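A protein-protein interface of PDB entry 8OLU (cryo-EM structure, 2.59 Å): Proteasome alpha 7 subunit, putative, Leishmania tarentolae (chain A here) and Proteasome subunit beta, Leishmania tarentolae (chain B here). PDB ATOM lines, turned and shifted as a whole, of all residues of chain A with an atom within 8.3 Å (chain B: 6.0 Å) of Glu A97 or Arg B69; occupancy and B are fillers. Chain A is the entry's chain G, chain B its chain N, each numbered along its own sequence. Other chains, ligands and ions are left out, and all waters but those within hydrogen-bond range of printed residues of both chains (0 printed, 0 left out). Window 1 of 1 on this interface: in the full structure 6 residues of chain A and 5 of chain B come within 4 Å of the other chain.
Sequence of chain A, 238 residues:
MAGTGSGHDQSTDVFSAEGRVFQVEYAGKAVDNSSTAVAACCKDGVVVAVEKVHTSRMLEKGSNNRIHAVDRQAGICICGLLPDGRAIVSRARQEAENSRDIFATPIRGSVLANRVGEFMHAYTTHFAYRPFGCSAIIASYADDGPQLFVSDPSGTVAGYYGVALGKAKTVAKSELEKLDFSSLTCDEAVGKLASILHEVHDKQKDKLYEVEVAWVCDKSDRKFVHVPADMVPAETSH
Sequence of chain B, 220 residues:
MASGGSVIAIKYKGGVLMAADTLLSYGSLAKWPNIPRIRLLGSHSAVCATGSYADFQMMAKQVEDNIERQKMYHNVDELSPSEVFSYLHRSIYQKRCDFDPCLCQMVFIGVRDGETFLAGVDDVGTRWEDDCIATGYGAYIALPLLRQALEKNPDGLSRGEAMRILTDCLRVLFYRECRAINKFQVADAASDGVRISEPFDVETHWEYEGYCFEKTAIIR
The side-chain carboxylate of Glu A97 lies within salt-bridge range of the guanidinium group of Arg B69.
OD1 of Asp A101 lies within salt-bridge range of NH2 of Arg B69 (3.0 Å).
The side-chain carboxylate of Glu A97 lies within hydrogen-bond range of the side-chain hydroxyl of Tyr B73 (2.5 Å).
The side-chain carboxylate of Asp A101 lies close to the side-chain carboxylate of Asp B65.
OD2 of Asp B65 lies within salt-bridge range of NH2 of Arg B69, 3.4 Å away.
NE of Arg A93 is in hydrogen-bond range of O of Ala A69 (3.0 Å).
The side-chain amide nitrogen (NE2) of Gln A73 lies within hydrogen-bond range of the side-chain carboxylate (OD2) of Asp A71, at 2.7 Å.
The side-chain carboxylate (OD2) of Asp A71 lies within salt-bridge range of the guanidinium group (NE) of Arg A100 (3.0 Å).
C of Asp A71 touches SD of Met B72 (3.6 Å).
NE of Arg A93 touches CD1 of Tyr B73, at 3.4 Å.
Glu A97 touches just these residues of chain B: Arg B69 (3.4 Å) and Tyr B73 (2.5 Å).
Arg B69 touches two residues of chain A.
Of the printed residues of chain A, Tyr B73 touches Arg A93 and Glu A97.
Of the printed residues of chain B, Asp A101 touches Asp B65 and Arg B69.
Of the printed residues of chain B, Asp A71 touches Met B72.
Val A89 touches none of the printed residues of chain B.
The nearest printed residue of chain B that does not touch Glu A97 is Asp B65 (6.2 Å).
The nearest residue of chain A that does not touch Arg B69 is Arg A100 (4.5 Å).
Of the 24 printed residues of chain A, 4 touch a printed residue of chain B.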
ATOM      1  N   ALA A  69      10.962  14.494 -10.424  1.00  0.00           N
ATOM      2  CA  ALA A  69      10.796  15.448 -11.502  1.00  0.00           C
ATOM      3  C   ALA A  69      11.145  14.821 -12.832  1.00  0.00           C
ATOM      4  O   ALA A  69      12.123  14.103 -12.981  1.00  0.00           O
ATOM      5  CB  ALA A  69      11.661  16.617 -11.260  1.00  0.00           C
ATOM      6  N   VAL A  70      10.417  15.231 -13.825  1.00  0.00           N
ATOM      7  CA  VAL A  70      10.637  14.734 -15.151  1.00  0.00           C
ATOM      8  C   VAL A  70      11.156  15.832 -16.055  1.00  0.00           C
ATOM      9  O   VAL A  70      11.746  15.573 -17.079  1.00  0.00           O
ATOM     10  CB  VAL A  70       9.271  14.272 -15.566  1.00  0.00           C
ATOM     11  CG1 VAL A  70       9.031  14.571 -16.991  1.00  0.00           C
ATOM     12  CG2 VAL A  70       9.110  12.809 -15.248  1.00  0.00           C
ATOM     13  N   ASP A  71      10.876  17.080 -15.722  1.00  0.00           N
ATOM     14  CA  ASP A  71      11.381  18.208 -16.448  1.00  0.00           C
ATOM     15  C   ASP A  71      11.266  19.368 -15.494  1.00  0.00           C
ATOM     16  O   ASP A  71      10.760  19.183 -14.401  1.00  0.00           O
ATOM     17  CB  ASP A  71      10.564  18.490 -17.694  1.00  0.00           C
ATOM     18  CG  ASP A  71      11.280  19.382 -18.733  1.00  0.00           C
ATOM     19  OD1 ASP A  71      12.529  19.759 -18.518  1.00  0.00           O
ATOM     20  OD2 ASP A  71      10.628  19.633 -19.882  1.00  0.00           O
ATOM     21  N   GLN A  73       9.119  21.610 -15.508  1.00  0.00           N
ATOM     22  CA  GLN A  73       7.764  21.998 -15.237  1.00  0.00           C
ATOM     23  C   GLN A  73       6.850  20.825 -14.967  1.00  0.00           C
ATOM     24  O   GLN A  73       5.648  20.965 -15.001  1.00  0.00           O
ATOM     25  CB  GLN A  73       7.265  22.722 -16.466  1.00  0.00           C
ATOM     26  CG  GLN A  73       6.984  21.886 -17.697  1.00  0.00           C
ATOM     27  CD  GLN A  73       8.238  21.429 -18.399  1.00  0.00           C
ATOM     28  OE1 GLN A  73       9.326  21.991 -18.195  1.00  0.00           O
ATOM     29  NE2 GLN A  73       8.099  20.389 -19.234  1.00  0.00           N
ATOM     30  N   VAL A  89       9.331   6.968 -15.250  1.00  0.00           N
ATOM     31  CA  VAL A  89      10.025   8.201 -15.021  1.00  0.00           C
ATOM     32  C   VAL A  89      11.213   8.308 -15.940  1.00  0.00           C
ATOM     33  O   VAL A  89      11.433   9.354 -16.522  1.00  0.00           O
ATOM     34  CB  VAL A  89      10.492   8.289 -13.577  1.00  0.00           C
ATOM     35  CG1 VAL A  89      11.434   9.462 -13.390  1.00  0.00           C
ATOM     36  CG2 VAL A  89       9.315   8.416 -12.616  1.00  0.00           C
ATOM     37  N   SER A  90      11.996   7.265 -16.110  1.00  0.00           N
ATOM     38  CA  SER A  90      13.045   7.438 -17.096  1.00  0.00           C
ATOM     39  C   SER A  90      12.493   7.658 -18.474  1.00  0.00           C
ATOM     40  O   SER A  90      12.994   8.526 -19.148  1.00  0.00           O
ATOM     41  CB  SER A  90      14.050   6.370 -17.120  1.00  0.00           C
ATOM     42  OG  SER A  90      14.651   6.323 -15.809  1.00  0.00           O
ATOM     43  N   ARG A  91      11.478   6.962 -18.873  1.00  0.00           N
ATOM     44  CA  ARG A  91      10.992   7.228 -20.188  1.00  0.00           C
ATOM     45  C   ARG A  91      10.372   8.622 -20.254  1.00  0.00           C
ATOM     46  O   ARG A  91      10.477   9.281 -21.286  1.00  0.00           O
ATOM     47  CB  ARG A  91      10.074   6.104 -20.635  1.00  0.00           C
ATOM     48  CG  ARG A  91       9.231   6.431 -21.860  1.00  0.00           C
ATOM     49  CD  ARG A  91       9.974   6.682 -23.157  1.00  0.00           C
ATOM     50  NE  ARG A  91      10.600   5.478 -23.636  1.00  0.00           N
ATOM     51  CZ  ARG A  91      10.166   4.861 -24.719  1.00  0.00           C
ATOM     52  NH1 ARG A  91      10.578   3.627 -24.999  1.00  0.00           N
ATOM     53  NH2 ARG A  91       9.258   5.482 -25.461  1.00  0.00           N
ATOM     54  N   ALA A  92       9.735   9.104 -19.180  1.00  0.00           N
ATOM     55  CA  ALA A  92       9.121  10.414 -19.304  1.00  0.00           C
ATOM     56  C   ALA A  92      10.190  11.467 -19.506  1.00  0.00           C
ATOM     57  O   ALA A  92      10.010  12.446 -20.163  1.00  0.00           O
ATOM     58  CB  ALA A  92       8.319  10.745 -18.098  1.00  0.00           C
ATOM     59  N   ARG A  93      11.323  11.239 -18.912  1.00  0.00           N
ATOM     60  CA  ARG A  93      12.393  12.177 -18.926  1.00  0.00           C
ATOM     61  C   ARG A  93      13.014  12.186 -20.266  1.00  0.00           C
ATOM     62  O   ARG A  93      13.480  13.205 -20.687  1.00  0.00           O
ATOM     63  CB  ARG A  93      13.461  11.739 -17.948  1.00  0.00           C
ATOM     64  CG  ARG A  93      13.028  11.999 -16.525  1.00  0.00           C
ATOM     65  CD  ARG A  93      14.090  11.596 -15.608  1.00  0.00           C
ATOM     66  NE  ARG A  93      13.703  11.914 -14.271  1.00  0.00           N
ATOM     67  CZ  ARG A  93      14.259  11.384 -13.226  1.00  0.00           C
ATOM     68  NH1 ARG A  93      15.133  10.419 -13.328  1.00  0.00           N
ATOM     69  NH2 ARG A  93      13.887  11.841 -12.063  1.00  0.00           N
ATOM     70  N   GLN A  94      12.993  11.065 -20.926  1.00  0.00           N
ATOM     71  CA  GLN A  94      13.565  11.033 -22.252  1.00  0.00           C
ATOM     72  C   GLN A  94      12.607  11.773 -23.172  1.00  0.00           C
ATOM     73  O   GLN A  94      13.012  12.435 -24.090  1.00  0.00           O
ATOM     74  CB  GLN A  94      13.872   9.573 -22.537  1.00  0.00           C
ATOM     75  CG  GLN A  94      14.238   9.256 -23.978  1.00  0.00           C
ATOM     76  CD  GLN A  94      14.212   7.750 -24.122  1.00  0.00           C
ATOM     77  OE1 GLN A  94      13.495   7.208 -24.969  1.00  0.00           O
ATOM     78  NE2 GLN A  94      14.909   7.075 -23.202  1.00  0.00           N
ATOM     79  N   GLU A  95      11.326  11.742 -22.905  1.00  0.00           N
ATOM     80  CA  GLU A  95      10.425  12.441 -23.779  1.00  0.00           C
ATOM     81  C   GLU A  95      10.542  13.933 -23.557  1.00  0.00           C
ATOM     82  O   GLU A  95      10.319  14.732 -24.461  1.00  0.00           O
ATOM     83  CB  GLU A  95       8.975  12.046 -23.547  1.00  0.00           C
ATOM     84  CG  GLU A  95       8.708  10.609 -23.920  1.00  0.00           C
ATOM     85  CD  GLU A  95       8.787  10.211 -25.397  1.00  0.00           C
ATOM     86  OE1 GLU A  95       8.665  11.135 -26.309  1.00  0.00           O
ATOM     87  OE2 GLU A  95       9.017   8.966 -25.651  1.00  0.00           O
ATOM     88  N   ALA A  96      10.743  14.301 -22.315  1.00  0.00           N
ATOM     89  CA  ALA A  96      10.852  15.686 -22.011  1.00  0.00           C
ATOM     90  C   ALA A  96      12.125  16.217 -22.614  1.00  0.00           C
ATOM     91  O   ALA A  96      12.159  17.318 -23.082  1.00  0.00           O
ATOM     92  CB  ALA A  96      10.844  15.857 -20.559  1.00  0.00           C
ATOM     93  N   GLU A  97      13.200  15.489 -22.485  1.00  0.00           N
ATOM     94  CA  GLU A  97      14.429  15.908 -23.091  1.00  0.00           C
ATOM     95  C   GLU A  97      14.223  16.017 -24.591  1.00  0.00           C
ATOM     96  O   GLU A  97      14.707  16.942 -25.206  1.00  0.00           O
ATOM     97  CB  GLU A  97      15.493  14.857 -22.887  1.00  0.00           C
ATOM     98  CG  GLU A  97      15.944  14.638 -21.453  1.00  0.00           C
ATOM     99  CD  GLU A  97      16.806  13.364 -21.250  1.00  0.00           C
ATOM    100  OE1 GLU A  97      17.022  12.912 -20.039  1.00  0.00           O
ATOM    101  OE2 GLU A  97      17.264  12.766 -22.318  1.00  0.00           O
ATOM    102  N   ASN A  98      13.566  15.046 -25.211  1.00  0.00           N
ATOM    103  CA  ASN A  98      13.410  15.091 -26.640  1.00  0.00           C
ATOM    104  C   ASN A  98      12.680  16.352 -27.005  1.00  0.00           C
ATOM    105  O   ASN A  98      13.069  17.022 -27.936  1.00  0.00           O
ATOM    106  CB  ASN A  98      12.646  13.936 -27.253  1.00  0.00           C
ATOM    107  CG  ASN A  98      13.388  12.620 -27.128  1.00  0.00           C
ATOM    108  OD1 ASN A  98      14.615  12.578 -26.925  1.00  0.00           O
ATOM    109  ND2 ASN A  98      12.618  11.527 -27.211  1.00  0.00           N
ATOM    110  N   SER A  99      11.642  16.693 -26.269  1.00  0.00           N
ATOM    111  CA  SER A  99      10.877  17.853 -26.645  1.00  0.00           C
ATOM    112  C   SER A  99      11.816  19.046 -26.604  1.00  0.00           C
ATOM    113  O   SER A  99      11.800  19.867 -27.492  1.00  0.00           O
ATOM    114  CB  SER A  99       9.645  18.038 -25.786  1.00  0.00           C
ATOM    115  OG  SER A  99       9.015  19.284 -26.119  1.00  0.00           O
ATOM    116  N   ARG A 100      12.688  19.147 -25.621  1.00  0.00           N
ATOM    117  CA  ARG A 100      13.563  20.302 -25.554  1.00  0.00           C
ATOM    118  C   ARG A 100      14.686  20.273 -26.582  1.00  0.00           C
ATOM    119  O   ARG A 100      15.114  21.320 -27.061  1.00  0.00           O
ATOM    120  CB  ARG A 100      14.154  20.433 -24.178  1.00  0.00           C
ATOM    121  CG  ARG A 100      13.152  21.146 -23.310  1.00  0.00           C
ATOM    122  CD  ARG A 100      13.684  21.081 -21.900  1.00  0.00           C
ATOM    123  NE  ARG A 100      12.664  21.534 -20.983  1.00  0.00           N
ATOM    124  CZ  ARG A 100      12.377  22.794 -20.739  1.00  0.00           C
ATOM    125  NH1 ARG A 100      13.002  23.787 -21.368  1.00  0.00           N
ATOM    126  NH2 ARG A 100      11.489  23.012 -19.795  1.00  0.00           N
ATOM    127  N   ASP A 101      15.130  19.085 -26.933  1.00  0.00           N
ATOM    128  CA  ASP A 101      16.298  18.965 -27.763  1.00  0.00           C
ATOM    129  C   ASP A 101      15.894  19.117 -29.221  1.00  0.00           C
ATOM    130  O   ASP A 101      16.423  19.963 -29.917  1.00  0.00           O
ATOM    131  CB  ASP A 101      17.060  17.710 -27.369  1.00  0.00           C
ATOM    132  CG  ASP A 101      17.627  17.812 -25.941  1.00  0.00           C
ATOM    133  OD1 ASP A 101      17.549  18.971 -25.365  1.00  0.00           O
ATOM    134  OD2 ASP A 101      18.191  16.754 -25.400  1.00  0.00           O
ATOM    135  N   ILE A 102      14.818  18.472 -29.611  1.00  0.00           N
ATOM    136  CA  ILE A 102      14.358  18.535 -30.973  1.00  0.00           C
ATOM    137  C   ILE A 102      13.418  19.699 -31.212  1.00  0.00           C
ATOM    138  O   ILE A 102      13.461  20.292 -32.272  1.00  0.00           O
ATOM    139  CB  ILE A 102      13.702  17.193 -31.296  1.00  0.00           C
ATOM    140  CG1 ILE A 102      14.734  16.065 -31.209  1.00  0.00           C
ATOM    141  CG2 ILE A 102      13.040  17.213 -32.627  1.00  0.00           C
ATOM    142  CD1 ILE A 102      14.141  14.720 -30.800  1.00  0.00           C
ATOM    143  N   PHE A 103      12.522  19.998 -30.305  1.00  0.00           N
ATOM    144  CA  PHE A 103      11.425  20.883 -30.625  1.00  0.00           C
ATOM    145  C   PHE A 103      11.605  22.196 -29.903  1.00  0.00           C
ATOM    146  O   PHE A 103      10.801  23.119 -30.075  1.00  0.00           O
ATOM    147  CB  PHE A 103      10.111  20.229 -30.241  1.00  0.00           C
ATOM    148  CG  PHE A 103       9.815  19.099 -31.161  1.00  0.00           C
ATOM    149  CD1 PHE A 103       9.531  19.338 -32.484  1.00  0.00           C
ATOM    150  CD2 PHE A 103       9.863  17.799 -30.741  1.00  0.00           C
ATOM    151  CE1 PHE A 103       9.280  18.305 -33.369  1.00  0.00           C
ATOM    152  CE2 PHE A 103       9.633  16.766 -31.644  1.00  0.00           C
ATOM    153  CZ  PHE A 103       9.356  17.018 -32.950  1.00  0.00           C
ATOM    154  N   ALA A 104      12.616  22.223 -29.045  1.00  0.00           N
ATOM    155  CA  ALA A 104      13.047  23.480 -28.435  1.00  0.00           C
ATOM    156  C   ALA A 104      11.911  24.128 -27.682  1.00  0.00           C
ATOM    157  O   ALA A 104      11.726  25.328 -27.797  1.00  0.00           O
ATOM    158  CB  ALA A 104      13.555  24.448 -29.486  1.00  0.00           C
ATOM    159  N   THR A 105      11.139  23.298 -27.011  1.00  0.00           N
ATOM    160  CA  THR A 105       9.978  23.734 -26.275  1.00  0.00           C
ATOM    161  C   THR A 105       9.892  22.749 -25.130  1.00  0.00           C
ATOM    162  O   THR A 105      10.167  21.562 -25.336  1.00  0.00           O
ATOM    163  CB  THR A 105       8.702  23.769 -27.170  1.00  0.00           C
ATOM    164  OG1 THR A 105       7.541  24.438 -26.635  1.00  0.00           O
ATOM    165  CG2 THR A 105       8.183  22.387 -27.557  1.00  0.00           C
ATOM    166  N   PRO A 106       9.423  23.177 -23.958  1.00  0.00           N
ATOM    167  CA  PRO A 106       9.008  22.246 -22.943  1.00  0.00           C
ATOM    168  C   PRO A 106       7.823  21.445 -23.401  1.00  0.00           C
ATOM    169  O   PRO A 106       6.935  21.986 -24.009  1.00  0.00           O
ATOM    170  CB  PRO A 106       8.484  23.101 -21.813  1.00  0.00           C
ATOM    171  CG  PRO A 106       9.125  24.442 -22.115  1.00  0.00           C
ATOM    172  CD  PRO A 106       9.062  24.549 -23.623  1.00  0.00           C
ATOM    173  N   ILE A 107       7.819  20.173 -23.038  1.00  0.00           N
ATOM    174  CA  ILE A 107       6.780  19.268 -23.443  1.00  0.00           C
ATOM    175  C   ILE A 107       5.517  19.724 -22.764  1.00  0.00           C
ATOM    176  O   ILE A 107       5.525  19.921 -21.568  1.00  0.00           O
ATOM    177  CB  ILE A 107       7.140  17.806 -23.097  1.00  0.00           C
ATOM    178  CG1 ILE A 107       6.213  16.821 -23.800  1.00  0.00           C
ATOM    179  CG2 ILE A 107       7.111  17.534 -21.608  1.00  0.00           C
ATOM    180  CD1 ILE A 107       6.743  15.432 -23.935  1.00  0.00           C
ATOM    181  N   LEU A 112       2.987  14.923 -22.647  1.00  0.00           N
ATOM    182  CA  LEU A 112       3.815  14.068 -21.822  1.00  0.00           C
ATOM    183  C   LEU A 112       3.040  12.884 -21.327  1.00  0.00           C
ATOM    184  O   LEU A 112       3.541  11.807 -21.279  1.00  0.00           O
ATOM    185  CB  LEU A 112       4.315  14.861 -20.620  1.00  0.00           C
ATOM    186  CG  LEU A 112       5.120  14.043 -19.644  1.00  0.00           C
ATOM    187  CD1 LEU A 112       6.288  13.408 -20.370  1.00  0.00           C
ATOM    188  CD2 LEU A 112       5.583  14.937 -18.519  1.00  0.00           C
ATOM    189  N   GLU B  64      25.014  22.268 -20.976  1.00  0.00           N
ATOM    190  CA  GLU B  64      23.986  22.864 -20.149  1.00  0.00           C
ATOM    191  C   GLU B  64      22.998  21.788 -19.736  1.00  0.00           C
ATOM    192  O   GLU B  64      22.575  21.746 -18.590  1.00  0.00           O
ATOM    193  CB  GLU B  64      23.147  23.893 -20.895  1.00  0.00           C
ATOM    194  CG  GLU B  64      23.362  25.354 -20.512  1.00  0.00           C
ATOM    195  CD  GLU B  64      22.883  26.401 -21.545  1.00  0.00           C
ATOM    196  OE1 GLU B  64      23.579  26.610 -22.599  1.00  0.00           O
ATOM    197  OE2 GLU B  64      21.811  27.035 -21.305  1.00  0.00           O
ATOM    198  N   ASP B  65      22.593  20.967 -20.703  1.00  0.00           N
ATOM    199  CA  ASP B  65      21.574  19.963 -20.490  1.00  0.00           C
ATOM    200  C   ASP B  65      22.064  18.897 -19.534  1.00  0.00           C
ATOM    201  O   ASP B  65      21.381  18.546 -18.589  1.00  0.00           O
ATOM    202  CB  ASP B  65      21.176  19.269 -21.783  1.00  0.00           C
ATOM    203  CG  ASP B  65      20.379  20.188 -22.714  1.00  0.00           C
ATOM    204  OD1 ASP B  65      20.110  21.405 -22.309  1.00  0.00           O
ATOM    205  OD2 ASP B  65      20.058  19.719 -23.885  1.00  0.00           O
ATOM    206  N   ASN B  66      23.256  18.412 -19.780  1.00  0.00           N
ATOM    207  CA  ASN B  66      23.868  17.450 -18.918  1.00  0.00           C
ATOM    208  C   ASN B  66      23.887  17.965 -17.500  1.00  0.00           C
ATOM    209  O   ASN B  66      23.518  17.286 -16.583  1.00  0.00           O
ATOM    210  CB  ASN B  66      25.252  17.175 -19.451  1.00  0.00           C
ATOM    211  CG  ASN B  66      25.971  16.113 -18.671  1.00  0.00           C
ATOM    212  OD1 ASN B  66      26.927  16.401 -17.963  1.00  0.00           O
ATOM    213  ND2 ASN B  66      25.458  14.907 -18.747  1.00  0.00           N
ATOM    214  N   ILE B  67      24.237  19.200 -17.311  1.00  0.00           N
ATOM    215  CA  ILE B  67      24.278  19.744 -15.977  1.00  0.00           C
ATOM    216  C   ILE B  67      22.911  19.754 -15.328  1.00  0.00           C
ATOM    217  O   ILE B  67      22.783  19.499 -14.149  1.00  0.00           O
ATOM    218  CB  ILE B  67      24.820  21.173 -16.010  1.00  0.00           C
ATOM    219  CG1 ILE B  67      26.257  21.187 -16.458  1.00  0.00           C
ATOM    220  CG2 ILE B  67      24.724  21.877 -14.676  1.00  0.00           C
ATOM    221  CD1 ILE B  67      26.748  22.605 -16.652  1.00  0.00           C
ATOM    222  N   GLU B  68      21.940  20.222 -16.071  1.00  0.00           N
ATOM    223  CA  GLU B  68      20.633  20.481 -15.543  1.00  0.00           C
ATOM    224  C   GLU B  68      19.929  19.159 -15.206  1.00  0.00           C
ATOM    225  O   GLU B  68      19.260  19.042 -14.187  1.00  0.00           O
ATOM    226  CB  GLU B  68      19.910  21.337 -16.587  1.00  0.00           C
ATOM    227  CG  GLU B  68      18.738  22.087 -15.992  1.00  0.00           C
ATOM    228  CD  GLU B  68      18.844  22.524 -14.514  1.00  0.00           C
ATOM    229  OE1 GLU B  68      19.378  23.674 -14.263  1.00  0.00           O
ATOM    230  OE2 GLU B  68      18.382  21.710 -13.588  1.00  0.00           O
ATOM    231  N   ARG B  69      20.089  18.180 -16.086  1.00  0.00           N
ATOM    232  CA  ARG B  69      19.476  16.900 -15.921  1.00  0.00           C
ATOM    233  C   ARG B  69      20.136  16.113 -14.813  1.00  0.00           C
ATOM    234  O   ARG B  69      19.483  15.446 -14.052  1.00  0.00           O
ATOM    235  CB  ARG B  69      19.614  16.132 -17.223  1.00  0.00           C
ATOM    236  CG  ARG B  69      18.743  16.747 -18.305  1.00  0.00           C
ATOM    237  CD  ARG B  69      18.956  16.198 -19.697  1.00  0.00           C
ATOM    238  NE  ARG B  69      18.285  17.153 -20.584  1.00  0.00           N
ATOM    239  CZ  ARG B  69      18.304  17.069 -21.923  1.00  0.00           C
ATOM    240  NH1 ARG B  69      19.023  16.126 -22.537  1.00  0.00           N
ATOM    241  NH2 ARG B  69      17.534  17.900 -22.606  1.00  0.00           N
ATOM    242  N   GLN B  70      21.446  16.145 -14.706  1.00  0.00           N
ATOM    243  CA  GLN B  70      22.108  15.409 -13.653  1.00  0.00           C
ATOM    244  C   GLN B  70      21.482  15.859 -12.350  1.00  0.00           C
ATOM    245  O   GLN B  70      21.239  15.056 -11.497  1.00  0.00           O
ATOM    246  CB  GLN B  70      23.617  15.631 -13.722  1.00  0.00           C
ATOM    247  CG  GLN B  70      24.429  14.492 -13.141  1.00  0.00           C
ATOM    248  CD  GLN B  70      25.350  14.860 -11.986  1.00  0.00           C
ATOM    249  OE1 GLN B  70      25.267  15.955 -11.407  1.00  0.00           O
ATOM    250  NE2 GLN B  70      26.214  13.912 -11.617  1.00  0.00           N
ATOM    251  N   LYS B  71      21.120  17.109 -12.240  1.00  0.00           N
ATOM    252  CA  LYS B  71      20.765  17.699 -10.979  1.00  0.00           C
ATOM    253  C   LYS B  71      19.277  17.585 -10.678  1.00  0.00           C
ATOM    254  O   LYS B  71      18.847  17.640  -9.528  1.00  0.00           O
ATOM    255  CB  LYS B  71      21.066  19.171 -11.178  1.00  0.00           C
ATOM    256  CG  LYS B  71      20.817  20.089 -10.007  1.00  0.00           C
ATOM    257  CD  LYS B  71      20.846  21.569 -10.387  1.00  0.00           C
ATOM    258  CE  LYS B  71      20.980  22.357  -9.091  1.00  0.00           C
ATOM    259  NZ  LYS B  71      20.064  23.517  -9.007  1.00  0.00           N
ATOM    260  N   MET B  72      18.471  17.577 -11.731  1.00  0.00           N
ATOM    261  CA  MET B  72      17.031  17.566 -11.616  1.00  0.00           C
ATOM    262  C   MET B  72      16.611  16.131 -11.395  1.00  0.00           C
ATOM    263  O   MET B  72      15.750  15.869 -10.560  1.00  0.00           O
ATOM    264  CB  MET B  72      16.447  18.127 -12.901  1.00  0.00           C
ATOM    265  CG  MET B  72      15.028  17.773 -13.328  1.00  0.00           C
ATOM    266  SD  MET B  72      14.789  18.547 -15.063  1.00  0.00           S
ATOM    267  CE  MET B  72      14.671  20.229 -14.478  1.00  0.00           C
ATOM    268  N   TYR B  73      17.308  15.228 -12.058  1.00  0.00           N
ATOM    269  CA  TYR B  73      16.973  13.833 -11.980  1.00  0.00           C
ATOM    270  C   TYR B  73      17.529  13.079 -10.794  1.00  0.00           C
ATOM    271  O   TYR B  73      17.079  11.980 -10.563  1.00  0.00           O
ATOM    272  CB  TYR B  73      17.580  13.044 -13.123  1.00  0.00           C
ATOM    273  CG  TYR B  73      17.094  13.413 -14.493  1.00  0.00           C
ATOM    274  CD1 TYR B  73      16.054  14.323 -14.684  1.00  0.00           C
ATOM    275  CD2 TYR B  73      17.680  12.818 -15.597  1.00  0.00           C
ATOM    276  CE1 TYR B  73      15.669  14.700 -15.967  1.00  0.00           C
ATOM    277  CE2 TYR B  73      17.282  13.164 -16.882  1.00  0.00           C
ATOM    278  CZ  TYR B  73      16.293  14.118 -17.061  1.00  0.00           C
ATOM    279  OH  TYR B  73      15.928  14.426 -18.342  1.00  0.00           O
ATOM    280  N   HIS B  74      18.616  13.514 -10.199  1.00  0.00           N
ATOM    281  CA  HIS B  74      19.147  12.852  -9.025  1.00  0.00           C
ATOM    282  C   HIS B  74      19.247  13.874  -7.906  1.00  0.00           C
ATOM    283  O   HIS B  74      19.337  15.069  -8.113  1.00  0.00           O
ATOM    284  CB  HIS B  74      20.475  12.225  -9.361  1.00  0.00           C
ATOM    285  CG  HIS B  74      20.481  11.382 -10.595  1.00  0.00           C
ATOM    286  ND1 HIS B  74      19.792  10.208 -10.722  1.00  0.00           N
ATOM    287  CD2 HIS B  74      21.157  11.586 -11.769  1.00  0.00           C
ATOM    288  CE1 HIS B  74      20.021   9.721 -11.955  1.00  0.00           C
ATOM    289  NE2 HIS B  74      20.859  10.567 -12.631  1.00  0.00           N
